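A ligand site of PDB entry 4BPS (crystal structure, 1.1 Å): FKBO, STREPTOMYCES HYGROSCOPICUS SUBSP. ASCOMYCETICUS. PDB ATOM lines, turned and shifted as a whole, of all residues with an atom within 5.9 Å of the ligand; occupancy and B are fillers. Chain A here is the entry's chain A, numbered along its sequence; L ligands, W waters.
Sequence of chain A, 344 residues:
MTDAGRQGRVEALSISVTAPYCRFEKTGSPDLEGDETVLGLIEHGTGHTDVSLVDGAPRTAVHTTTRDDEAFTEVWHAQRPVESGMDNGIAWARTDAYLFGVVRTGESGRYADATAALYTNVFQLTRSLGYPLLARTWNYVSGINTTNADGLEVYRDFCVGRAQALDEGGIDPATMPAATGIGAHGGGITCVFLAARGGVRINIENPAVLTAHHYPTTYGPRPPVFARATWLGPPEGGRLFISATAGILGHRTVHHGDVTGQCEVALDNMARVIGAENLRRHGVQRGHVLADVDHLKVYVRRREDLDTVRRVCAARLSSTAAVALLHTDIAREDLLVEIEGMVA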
ATOM      1  N   THR A 137     -22.505  23.863 -34.749  1.00  0.00           N
ATOM      2  CA  THR A 137     -22.630  22.668 -33.942  1.00  0.00           C
ATOM      3  C   THR A 137     -24.103  22.369 -33.698  1.00  0.00           C
ATOM      4  O   THR A 137     -24.942  23.280 -33.685  1.00  0.00           O
ATOM      5  CB  THR A 137     -21.920  22.815 -32.563  1.00  0.00           C
ATOM      6  OG1 THR A 137     -22.549  23.849 -31.804  1.00  0.00           O
ATOM      7  CG2 THR A 137     -20.439  23.078 -32.727  1.00  0.00           C
ATOM      8  N   ASN A 139     -26.495  19.783 -30.942  1.00  0.00           N
ATOM      9  CA  ASN A 139     -26.539  18.881 -29.788  1.00  0.00           C
ATOM     10  C   ASN A 139     -27.960  18.375 -29.656  1.00  0.00           C
ATOM     11  O   ASN A 139     -28.888  19.149 -29.386  1.00  0.00           O
ATOM     12  CB  ASN A 139     -26.128  19.614 -28.505  1.00  0.00           C
ATOM     13  CG  ASN A 139     -24.821  20.360 -28.648  1.00  0.00           C
ATOM     14  OD1 ASN A 139     -23.761  19.773 -28.544  1.00  0.00           O
ATOM     15  ND2 ASN A 139     -24.905  21.673 -28.926  1.00  0.00           N
ATOM     16  N   TYR A 155     -30.274  19.376 -19.385  1.00  0.00           N
ATOM     17  CA  TYR A 155     -29.678  20.469 -20.186  1.00  0.00           C
ATOM     18  C   TYR A 155     -28.557  21.164 -19.407  1.00  0.00           C
ATOM     19  O   TYR A 155     -27.540  21.542 -19.979  1.00  0.00           O
ATOM     20  CB  TYR A 155     -30.742  21.503 -20.542  1.00  0.00           C
ATOM     21  CG  TYR A 155     -30.172  22.653 -21.369  1.00  0.00           C
ATOM     22  CD1 TYR A 155     -29.607  22.430 -22.630  1.00  0.00           C
ATOM     23  CD2 TYR A 155     -30.161  23.949 -20.883  1.00  0.00           C
ATOM     24  CE1 TYR A 155     -29.071  23.456 -23.368  1.00  0.00           C
ATOM     25  CE2 TYR A 155     -29.670  24.994 -21.625  1.00  0.00           C
ATOM     26  CZ  TYR A 155     -29.111  24.747 -22.855  1.00  0.00           C
ATOM     27  OH  TYR A 155     -28.600  25.801 -23.574  1.00  0.00           O
ATOM     28  N   PHE A 158     -25.481  18.922 -19.304  1.00  0.00           N
ATOM     29  CA  PHE A 158     -24.844  19.085 -20.608  1.00  0.00           C
ATOM     30  C   PHE A 158     -24.061  20.404 -20.682  1.00  0.00           C
ATOM     31  O   PHE A 158     -22.923  20.429 -21.160  1.00  0.00           O
ATOM     32  CB  PHE A 158     -25.933  19.002 -21.699  1.00  0.00           C
ATOM     33  CG  PHE A 158     -25.509  19.625 -23.005  1.00  0.00           C
ATOM     34  CD1 PHE A 158     -24.620  18.970 -23.855  1.00  0.00           C
ATOM     35  CD2 PHE A 158     -25.988  20.870 -23.375  1.00  0.00           C
ATOM     36  CE1 PHE A 158     -24.192  19.564 -25.030  1.00  0.00           C
ATOM     37  CE2 PHE A 158     -25.572  21.461 -24.567  1.00  0.00           C
ATOM     38  CZ  PHE A 158     -24.663  20.800 -25.381  1.00  0.00           C
ATOM     39  N   CYS A 159     -24.672  21.516 -20.240  1.00  0.00           N
ATOM     40  CA  CYS A 159     -23.971  22.789 -20.300  1.00  0.00           C
ATOM     41  C   CYS A 159     -22.708  22.783 -19.453  1.00  0.00           C
ATOM     42  O   CYS A 159     -21.708  23.415 -19.835  1.00  0.00           O
ATOM     43  CB  CYS A 159     -24.883  23.941 -19.853  1.00  0.00           C
ATOM     44  SG  CYS A 159     -26.094  24.478 -21.117  1.00  0.00           S
ATOM     45  N   ARG A 162     -20.046  20.909 -21.580  1.00  0.00           N
ATOM     46  CA  ARG A 162     -19.560  21.709 -22.694  1.00  0.00           C
ATOM     47  C   ARG A 162     -18.629  22.811 -22.199  1.00  0.00           C
ATOM     48  O   ARG A 162     -17.547  23.005 -22.741  1.00  0.00           O
ATOM     49  CB  ARG A 162     -20.755  22.254 -23.475  1.00  0.00           C
ATOM     50  CG  ARG A 162     -20.359  23.241 -24.558  1.00  0.00           C
ATOM     51  CD  ARG A 162     -21.516  23.604 -25.496  1.00  0.00           C
ATOM     52  NE  ARG A 162     -22.633  24.237 -24.758  1.00  0.00           N
ATOM     53  CZ  ARG A 162     -23.818  24.511 -25.302  1.00  0.00           C
ATOM     54  NH1 ARG A 162     -24.073  24.253 -26.593  1.00  0.00           N
ATOM     55  NH2 ARG A 162     -24.771  25.054 -24.540  1.00  0.00           N
ATOM     56  N   ALA A 179     -25.325  27.284 -33.025  1.00  0.00           N
ATOM     57  CA  ALA A 179     -25.588  26.024 -32.339  1.00  0.00           C
ATOM     58  C   ALA A 179     -27.070  25.723 -32.246  1.00  0.00           C
ATOM     59  O   ALA A 179     -27.939  26.588 -32.444  1.00  0.00           O
ATOM     60  CB  ALA A 179     -24.982  26.051 -30.922  1.00  0.00           C
ATOM     61  N   THR A 180     -27.341  24.462 -31.934  1.00  0.00           N
ATOM     62  CA  THR A 180     -28.640  23.967 -31.500  1.00  0.00           C
ATOM     63  C   THR A 180     -28.442  23.109 -30.270  1.00  0.00           C
ATOM     64  O   THR A 180     -27.497  22.327 -30.224  1.00  0.00           O
ATOM     65  CB  THR A 180     -29.259  23.114 -32.604  1.00  0.00           C
ATOM     66  OG1 THR A 180     -29.511  23.977 -33.721  1.00  0.00           O
ATOM     67  CG2 THR A 180     -30.547  22.426 -32.176  1.00  0.00           C
ATOM     68  N   GLY A 181     -29.326  23.282 -29.280  1.00  0.00           N
ATOM     69  CA  GLY A 181     -29.365  22.453 -28.076  1.00  0.00           C
ATOM     70  C   GLY A 181     -30.803  22.023 -27.890  1.00  0.00           C
ATOM     71  O   GLY A 181     -31.626  22.794 -27.376  1.00  0.00           O
ATOM     72  N   VAL A 209     -30.878  40.197 -27.808  1.00  0.00           N
ATOM     73  CA  VAL A 209     -30.777  38.917 -27.108  1.00  0.00           C
ATOM     74  C   VAL A 209     -29.425  38.859 -26.442  1.00  0.00           C
ATOM     75  O   VAL A 209     -28.401  39.176 -27.054  1.00  0.00           O
ATOM     76  CB  VAL A 209     -30.992  37.718 -28.069  1.00  0.00           C
ATOM     77  CG1 VAL A 209     -30.732  36.395 -27.368  1.00  0.00           C
ATOM     78  CG2 VAL A 209     -32.438  37.738 -28.607  1.00  0.00           C
ATOM     79  N   ALA A 212     -25.202  34.163 -25.036  1.00  0.00           N
ATOM     80  CA  ALA A 212     -25.524  32.955 -24.260  1.00  0.00           C
ATOM     81  C   ALA A 212     -24.600  32.789 -23.060  1.00  0.00           C
ATOM     82  O   ALA A 212     -25.071  32.514 -21.950  1.00  0.00           O
ATOM     83  CB  ALA A 212     -25.511  31.732 -25.172  1.00  0.00           C
ATOM     84  N   TYR A 215     -25.470  34.616 -19.898  1.00  0.00           N
ATOM     85  CA  TYR A 215     -26.698  34.384 -19.167  1.00  0.00           C
ATOM     86  C   TYR A 215     -26.448  34.383 -17.653  1.00  0.00           C
ATOM     87  O   TYR A 215     -25.425  33.888 -17.178  1.00  0.00           O
ATOM     88  CB  TYR A 215     -27.327  33.042 -19.543  1.00  0.00           C
ATOM     89  CG  TYR A 215     -28.108  32.943 -20.850  1.00  0.00           C
ATOM     90  CD1 TYR A 215     -28.195  34.008 -21.756  1.00  0.00           C
ATOM     91  CD2 TYR A 215     -28.747  31.768 -21.176  1.00  0.00           C
ATOM     92  CE1 TYR A 215     -28.912  33.861 -22.925  1.00  0.00           C
ATOM     93  CE2 TYR A 215     -29.454  31.593 -22.348  1.00  0.00           C
ATOM     94  CZ  TYR A 215     -29.534  32.649 -23.235  1.00  0.00           C
ATOM     95  OH  TYR A 215     -30.210  32.533 -24.447  1.00  0.00           O
ATOM     96  N   PRO A 224     -24.964  28.342 -21.066  1.00  0.00           N
ATOM     97  CA  PRO A 224     -24.736  27.890 -22.439  1.00  0.00           C
ATOM     98  C   PRO A 224     -23.697  28.757 -23.116  1.00  0.00           C
ATOM     99  O   PRO A 224     -23.354  29.836 -22.623  1.00  0.00           O
ATOM    100  CB  PRO A 224     -26.110  28.036 -23.111  1.00  0.00           C
ATOM    101  CG  PRO A 224     -26.996  28.694 -22.138  1.00  0.00           C
ATOM    102  CD  PRO A 224     -26.249  29.023 -20.890  1.00  0.00           C
ATOM    103  N   VAL A 225     -23.170  28.276 -24.243  1.00  0.00           N
ATOM    104  CA  VAL A 225     -22.234  29.069 -25.039  1.00  0.00           C
ATOM    105  C   VAL A 225     -22.476  28.743 -26.496  1.00  0.00           C
ATOM    106  O   VAL A 225     -22.517  27.574 -26.870  1.00  0.00           O
ATOM    107  CB  VAL A 225     -20.767  28.800 -24.627  1.00  0.00           C
ATOM    108  CG1 VAL A 225     -20.404  27.293 -24.685  1.00  0.00           C
ATOM    109  CG2 VAL A 225     -19.809  29.604 -25.457  1.00  0.00           C
ATOM    110  N   PHE A 226     -22.680  29.795 -27.289  1.00  0.00           N
ATOM    111  CA  PHE A 226     -22.935  29.679 -28.737  1.00  0.00           C
ATOM    112  C   PHE A 226     -23.199  31.063 -29.312  1.00  0.00           C
ATOM    113  O   PHE A 226     -23.706  31.949 -28.604  1.00  0.00           O
ATOM    114  CB  PHE A 226     -24.113  28.730 -29.094  1.00  0.00           C
ATOM    115  CG  PHE A 226     -25.442  29.099 -28.468  1.00  0.00           C
ATOM    116  CD1 PHE A 226     -25.813  28.618 -27.218  1.00  0.00           C
ATOM    117  CD2 PHE A 226     -26.318  29.920 -29.145  1.00  0.00           C
ATOM    118  CE1 PHE A 226     -27.030  28.943 -26.663  1.00  0.00           C
ATOM    119  CE2 PHE A 226     -27.542  30.256 -28.592  1.00  0.00           C
ATOM    120  CZ  PHE A 226     -27.886  29.786 -27.347  1.00  0.00           C
ATOM    121  N   ARG A 228     -25.304  33.455 -32.227  1.00  0.00           N
ATOM    122  CA  ARG A 228     -26.685  33.449 -32.723  1.00  0.00           C
ATOM    123  C   ARG A 228     -26.747  33.119 -34.241  1.00  0.00           C
ATOM    124  O   ARG A 228     -27.794  32.652 -34.730  1.00  0.00           O
ATOM    125  CB  ARG A 228     -27.402  34.765 -32.392  1.00  0.00           C
ATOM    126  CG  ARG A 228     -27.406  35.045 -30.894  1.00  0.00           C
ATOM    127  CD  ARG A 228     -28.226  34.015 -30.129  1.00  0.00           C
ATOM    128  NE  ARG A 228     -28.008  34.154 -28.698  1.00  0.00           N
ATOM    129  CZ  ARG A 228     -28.789  33.558 -27.785  1.00  0.00           C
ATOM    130  NH1 ARG A 228     -29.815  32.818 -28.159  1.00  0.00           N
ATOM    131  NH2 ARG A 228     -28.526  33.733 -26.495  1.00  0.00           N
ATOM    132  N   SER A 243     -28.501  29.831 -35.788  1.00  0.00           N
ATOM    133  CA  SER A 243     -28.731  28.937 -34.644  1.00  0.00           C
ATOM    134  C   SER A 243     -30.194  28.576 -34.514  1.00  0.00           C
ATOM    135  O   SER A 243     -31.067  29.295 -35.021  1.00  0.00           O
ATOM    136  CB  SER A 243     -28.281  29.627 -33.367  1.00  0.00           C
ATOM    137  OG  SER A 243     -26.869  29.748 -33.400  1.00  0.00           O
ATOM    138  N   ALA A 244     -30.477  27.503 -33.771  1.00  0.00           N
ATOM    139  CA  ALA A 244     -31.822  27.320 -33.261  1.00  0.00           C
ATOM    140  C   ALA A 244     -32.195  28.580 -32.492  1.00  0.00           C
ATOM    141  O   ALA A 244     -31.431  29.036 -31.625  1.00  0.00           O
ATOM    142  CB  ALA A 244     -31.885  26.112 -32.368  1.00  0.00           C
ATOM    143  N   THR A 245     -33.351  29.142 -32.825  1.00  0.00           N
ATOM    144  CA  THR A 245     -33.776  30.461 -32.346  1.00  0.00           C
ATOM    145  C   THR A 245     -35.134  30.348 -31.653  1.00  0.00           C
ATOM    146  O   THR A 245     -36.060  29.762 -32.221  1.00  0.00           O
ATOM    147  CB  THR A 245     -33.855  31.415 -33.553  1.00  0.00           C
ATOM    148  OG1 THR A 245     -32.578  31.466 -34.219  1.00  0.00           O
ATOM    149  CG2 THR A 245     -34.218  32.837 -33.083  1.00  0.00           C
ATOM    150  N   ALA A 246     -35.200  30.881 -30.439  1.00  0.00           N
ATOM    151  CA  ALA A 246     -36.358  30.755 -29.566  1.00  0.00           C
ATOM    152  C   ALA A 246     -37.066  32.093 -29.358  1.00  0.00           C
ATOM    153  O   ALA A 246     -36.561  33.161 -29.736  1.00  0.00           O
ATOM    154  CB  ALA A 246     -35.910  30.215 -28.210  1.00  0.00           C
ATOM    155  N   ILE A 248     -37.323  34.415 -27.105  1.00  0.00           N
ATOM    156  CA  ILE A 248     -36.626  35.036 -25.993  1.00  0.00           C
ATOM    157  C   ILE A 248     -36.359  36.507 -26.343  1.00  0.00           C
ATOM    158  O   ILE A 248     -36.120  36.854 -27.509  1.00  0.00           O
ATOM    159  CB  ILE A 248     -35.271  34.279 -25.738  1.00  0.00           C
ATOM    160  CG1 ILE A 248     -35.493  32.987 -24.942  1.00  0.00           C
ATOM    161  CG2 ILE A 248     -34.247  35.125 -25.010  1.00  0.00           C
ATOM    162  CD1 ILE A 248     -34.314  32.011 -24.961  1.00  0.00           C
ATOM    163  N   ILE A 330     -37.502  21.378 -25.947  1.00  0.00           N
ATOM    164  CA  ILE A 330     -36.599  22.500 -26.096  1.00  0.00           C
ATOM    165  C   ILE A 330     -35.736  22.644 -24.820  1.00  0.00           C
ATOM    166  O   ILE A 330     -36.064  22.086 -23.762  1.00  0.00           O
ATOM    167  CB  ILE A 330     -37.402  23.816 -26.339  1.00  0.00           C
ATOM    168  CG1 ILE A 330     -38.646  23.566 -27.230  1.00  0.00           C
ATOM    169  CG2 ILE A 330     -36.485  24.949 -26.879  1.00  0.00           C
ATOM    170  CD1 ILE A 330     -38.349  23.161 -28.675  1.00  0.00           C
ATOM    171  N   ALA A 331     -34.638  23.402 -24.893  1.00  0.00           N
ATOM    172  CA  ALA A 331     -33.677  23.475 -23.790  1.00  0.00           C
ATOM    173  C   ALA A 331     -34.254  23.960 -22.461  1.00  0.00           C
ATOM    174  O   ALA A 331     -33.729  23.558 -21.421  1.00  0.00           O
ATOM    175  CB  ALA A 331     -32.518  24.399 -24.188  1.00  0.00           C
ATOM    176  N   ARG A 332     -35.273  24.840 -22.499  1.00  0.00           N
ATOM    177  CA  ARG A 332     -36.013  25.210 -21.287  1.00  0.00           C
ATOM    178  C   ARG A 332     -37.413  24.640 -21.391  1.00  0.00           C
ATOM    179  O   ARG A 332     -38.025  24.703 -22.470  1.00  0.00           O
ATOM    180  CB  ARG A 332     -36.188  26.724 -21.145  1.00  0.00           C
ATOM    181  CG  ARG A 332     -34.917  27.501 -21.148  1.00  0.00           C
ATOM    182  CD  ARG A 332     -35.198  28.969 -21.093  1.00  0.00           C
ATOM    183  NE  ARG A 332     -33.957  29.723 -21.164  1.00  0.00           N
ATOM    184  CZ  ARG A 332     -33.885  31.042 -21.267  1.00  0.00           C
ATOM    185  NH1 ARG A 332     -34.989  31.805 -21.382  1.00  0.00           N
ATOM    186  NH2 ARG A 332     -32.686  31.608 -21.288  1.00  0.00           N
ATOM    187  N   LEU A 335     -39.946  26.938 -23.058  1.00  0.00           N
ATOM    188  CA  LEU A 335     -39.846  27.199 -24.487  1.00  0.00           C
ATOM    189  C   LEU A 335     -40.614  26.124 -25.216  1.00  0.00           C
ATOM    190  O   LEU A 335     -40.470  24.924 -24.937  1.00  0.00           O
ATOM    191  CB  LEU A 335     -38.387  27.273 -24.932  1.00  0.00           C
ATOM    192  CG  LEU A 335     -37.602  28.452 -24.343  1.00  0.00           C
ATOM    193  CD1 LEU A 335     -36.120  28.322 -24.687  1.00  0.00           C
ATOM    194  CD2 LEU A 335     -38.159  29.811 -24.806  1.00  0.00           C
ATOM    195  N   GLU A 338     -38.749  26.223 -31.501  1.00  0.00           N
ATOM    196  CA  GLU A 338     -37.551  26.894 -31.972  1.00  0.00           C
ATOM    197  C   GLU A 338     -37.379  26.629 -33.463  1.00  0.00           C
ATOM    198  O   GLU A 338     -37.891  25.620 -33.972  1.00  0.00           O
ATOM    199  CB  GLU A 338     -36.299  26.383 -31.292  1.00  0.00           C
ATOM    200  CG  GLU A 338     -36.130  26.840 -29.894  1.00  0.00           C
ATOM    201  CD  GLU A 338     -34.784  26.436 -29.356  1.00  0.00           C
ATOM    202  OE1 GLU A 338     -34.222  25.405 -29.840  1.00  0.00           O
ATOM    203  OE2 GLU A 338     -34.254  27.113 -28.469  1.00  0.00           O
HETATM  204  C1  LIG L   1     -31.583  30.081 -26.128  1.00  0.00           C
HETATM  205  O1  LIG L   1     -30.884  30.033 -25.111  1.00  0.00           O
HETATM  206  C2  LIG L   1     -32.516  28.967 -26.517  1.00  0.00           C
HETATM  207  O2  LIG L   1     -27.339  25.097 -25.722  1.00  0.00           O
HETATM  208  O3  LIG L   1     -26.535  24.835 -27.771  1.00  0.00           O
HETATM  209  C3  LIG L   1     -30.560  27.755 -28.525  1.00  0.00           C
HETATM  210  C4  LIG L   1     -29.482  27.417 -29.323  1.00  0.00           C
HETATM  211  C5  LIG L   1     -30.656  27.277 -27.215  1.00  0.00           C
HETATM  212  C6  LIG L   1     -28.485  26.583 -28.832  1.00  0.00           C
HETATM  213  C7  LIG L   1     -27.432  25.287 -26.949  1.00  0.00           C
HETATM  214  C8  LIG L   1     -29.639  26.465 -26.731  1.00  0.00           C
HETATM  215  C9  LIG L   1     -28.533  26.122 -27.521  1.00  0.00           C
HETATM  216  O4  LIG L   1     -31.616  31.119 -26.889  1.00  0.00           O
HETATM  217  C10 LIG L   1     -31.854  27.578 -26.331  1.00  0.00           C
HETATM  218  O   HOH W   1     -31.783  24.890 -28.974  1.00  0.00           O
HETATM  219  O   HOH W   2     -32.754  31.747 -29.202  1.00  0.00           O
HETATM  220  O   HOH W   3     -30.273  28.130 -23.212  1.00  0.00           O
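Residues that only touch the ligand: Glu 338 (3.2 Å), Phe 226 (3.3 Å), Ala 244 (3.4 Å), Gly 181 (3.4 Å), Ile 248 (3.4 Å), Ala 179 (3.6 Å), Thr 180 (3.6 Å), Asn 139 (3.7 Å), Ala 331 (3.9 Å) and Ala 246 (3.99 Å). Hydrophobic or aromatic side chains that line the ligand: Tyr 155, Ala 179, Tyr 215, Phe 226, Ala 246, Ile 248 and Ala 331. 14 residues have an atom within 4 Å of the ligand: Asn 139, Tyr 155, Arg 162, Ala 179, Thr 180, Gly 181, Tyr 215, Phe 226, Arg 228, Ala 244, Ala 246, Ile 248, Ala 331 and Glu 338. The nearest printed residue that does not touch the ligand is Leu 335 (4.1 Å).
The backbone NH of Ser 243 sits at hydrogen-bond distance from the backbone carbonyl oxygen of Arg 228, 3.1 Å away. O of Tyr 155 sits at hydrogen-bond distance from SG of Cys 159 (3.5 Å). OH of Tyr 215 lies within hydrogen-bond range of NH2 of Arg 228 (2.9 Å). The backbone NH (N) of Ala 179 sits at hydrogen-bond distance from the side-chain hydroxyl (OG) of Ser 243, 2.9 Å away. The backbone carbonyl oxygen of Thr 180 sits at hydrogen-bond distance from the backbone NH of Asn 139, at 2.8 Å. O of Thr 137 is in hydrogen-bond range of N of Thr 180 (3.2 Å). The guanidinium group of Arg 162 lies within hydrogen-bond range of the side-chain sulfur of Cys 159 (3.7 Å). The backbone NH of Ala 244 sits at hydrogen-bond distance from the backbone carbonyl oxygen of Ala 179 (3.0 Å).
The guanidinium group (NH1) of Arg 162 is in salt-bridge range of an oxygen (O3) of the ligand. The side-chain hydroxyl (OH) of Tyr 155 lies within hydrogen-bond range of an oxygen (O2) of the ligand, 2.6 Å away. The guanidinium group of Arg 228 lies within salt-bridge range of an oxygen (O4) of the ligand, 2.8 Å away. An oxygen (O1) of the ligand lies within hydrogen-bond range of the side-chain hydroxyl (OH) of Tyr 215 (2.7 Å).
Water W2 lies within hydrogen-bond range of an oxygen (O4) of the ligand, the backbone NH (N) of Ala 246 and the guanidinium group (NH1) of Arg 228. Water W3 lies within hydrogen-bond range of O1 of the ligand (2.8 Å) and OH of Tyr 155 (2.9 Å). Water W1 bridges OE1 of Glu 338 and O of Gly 181.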
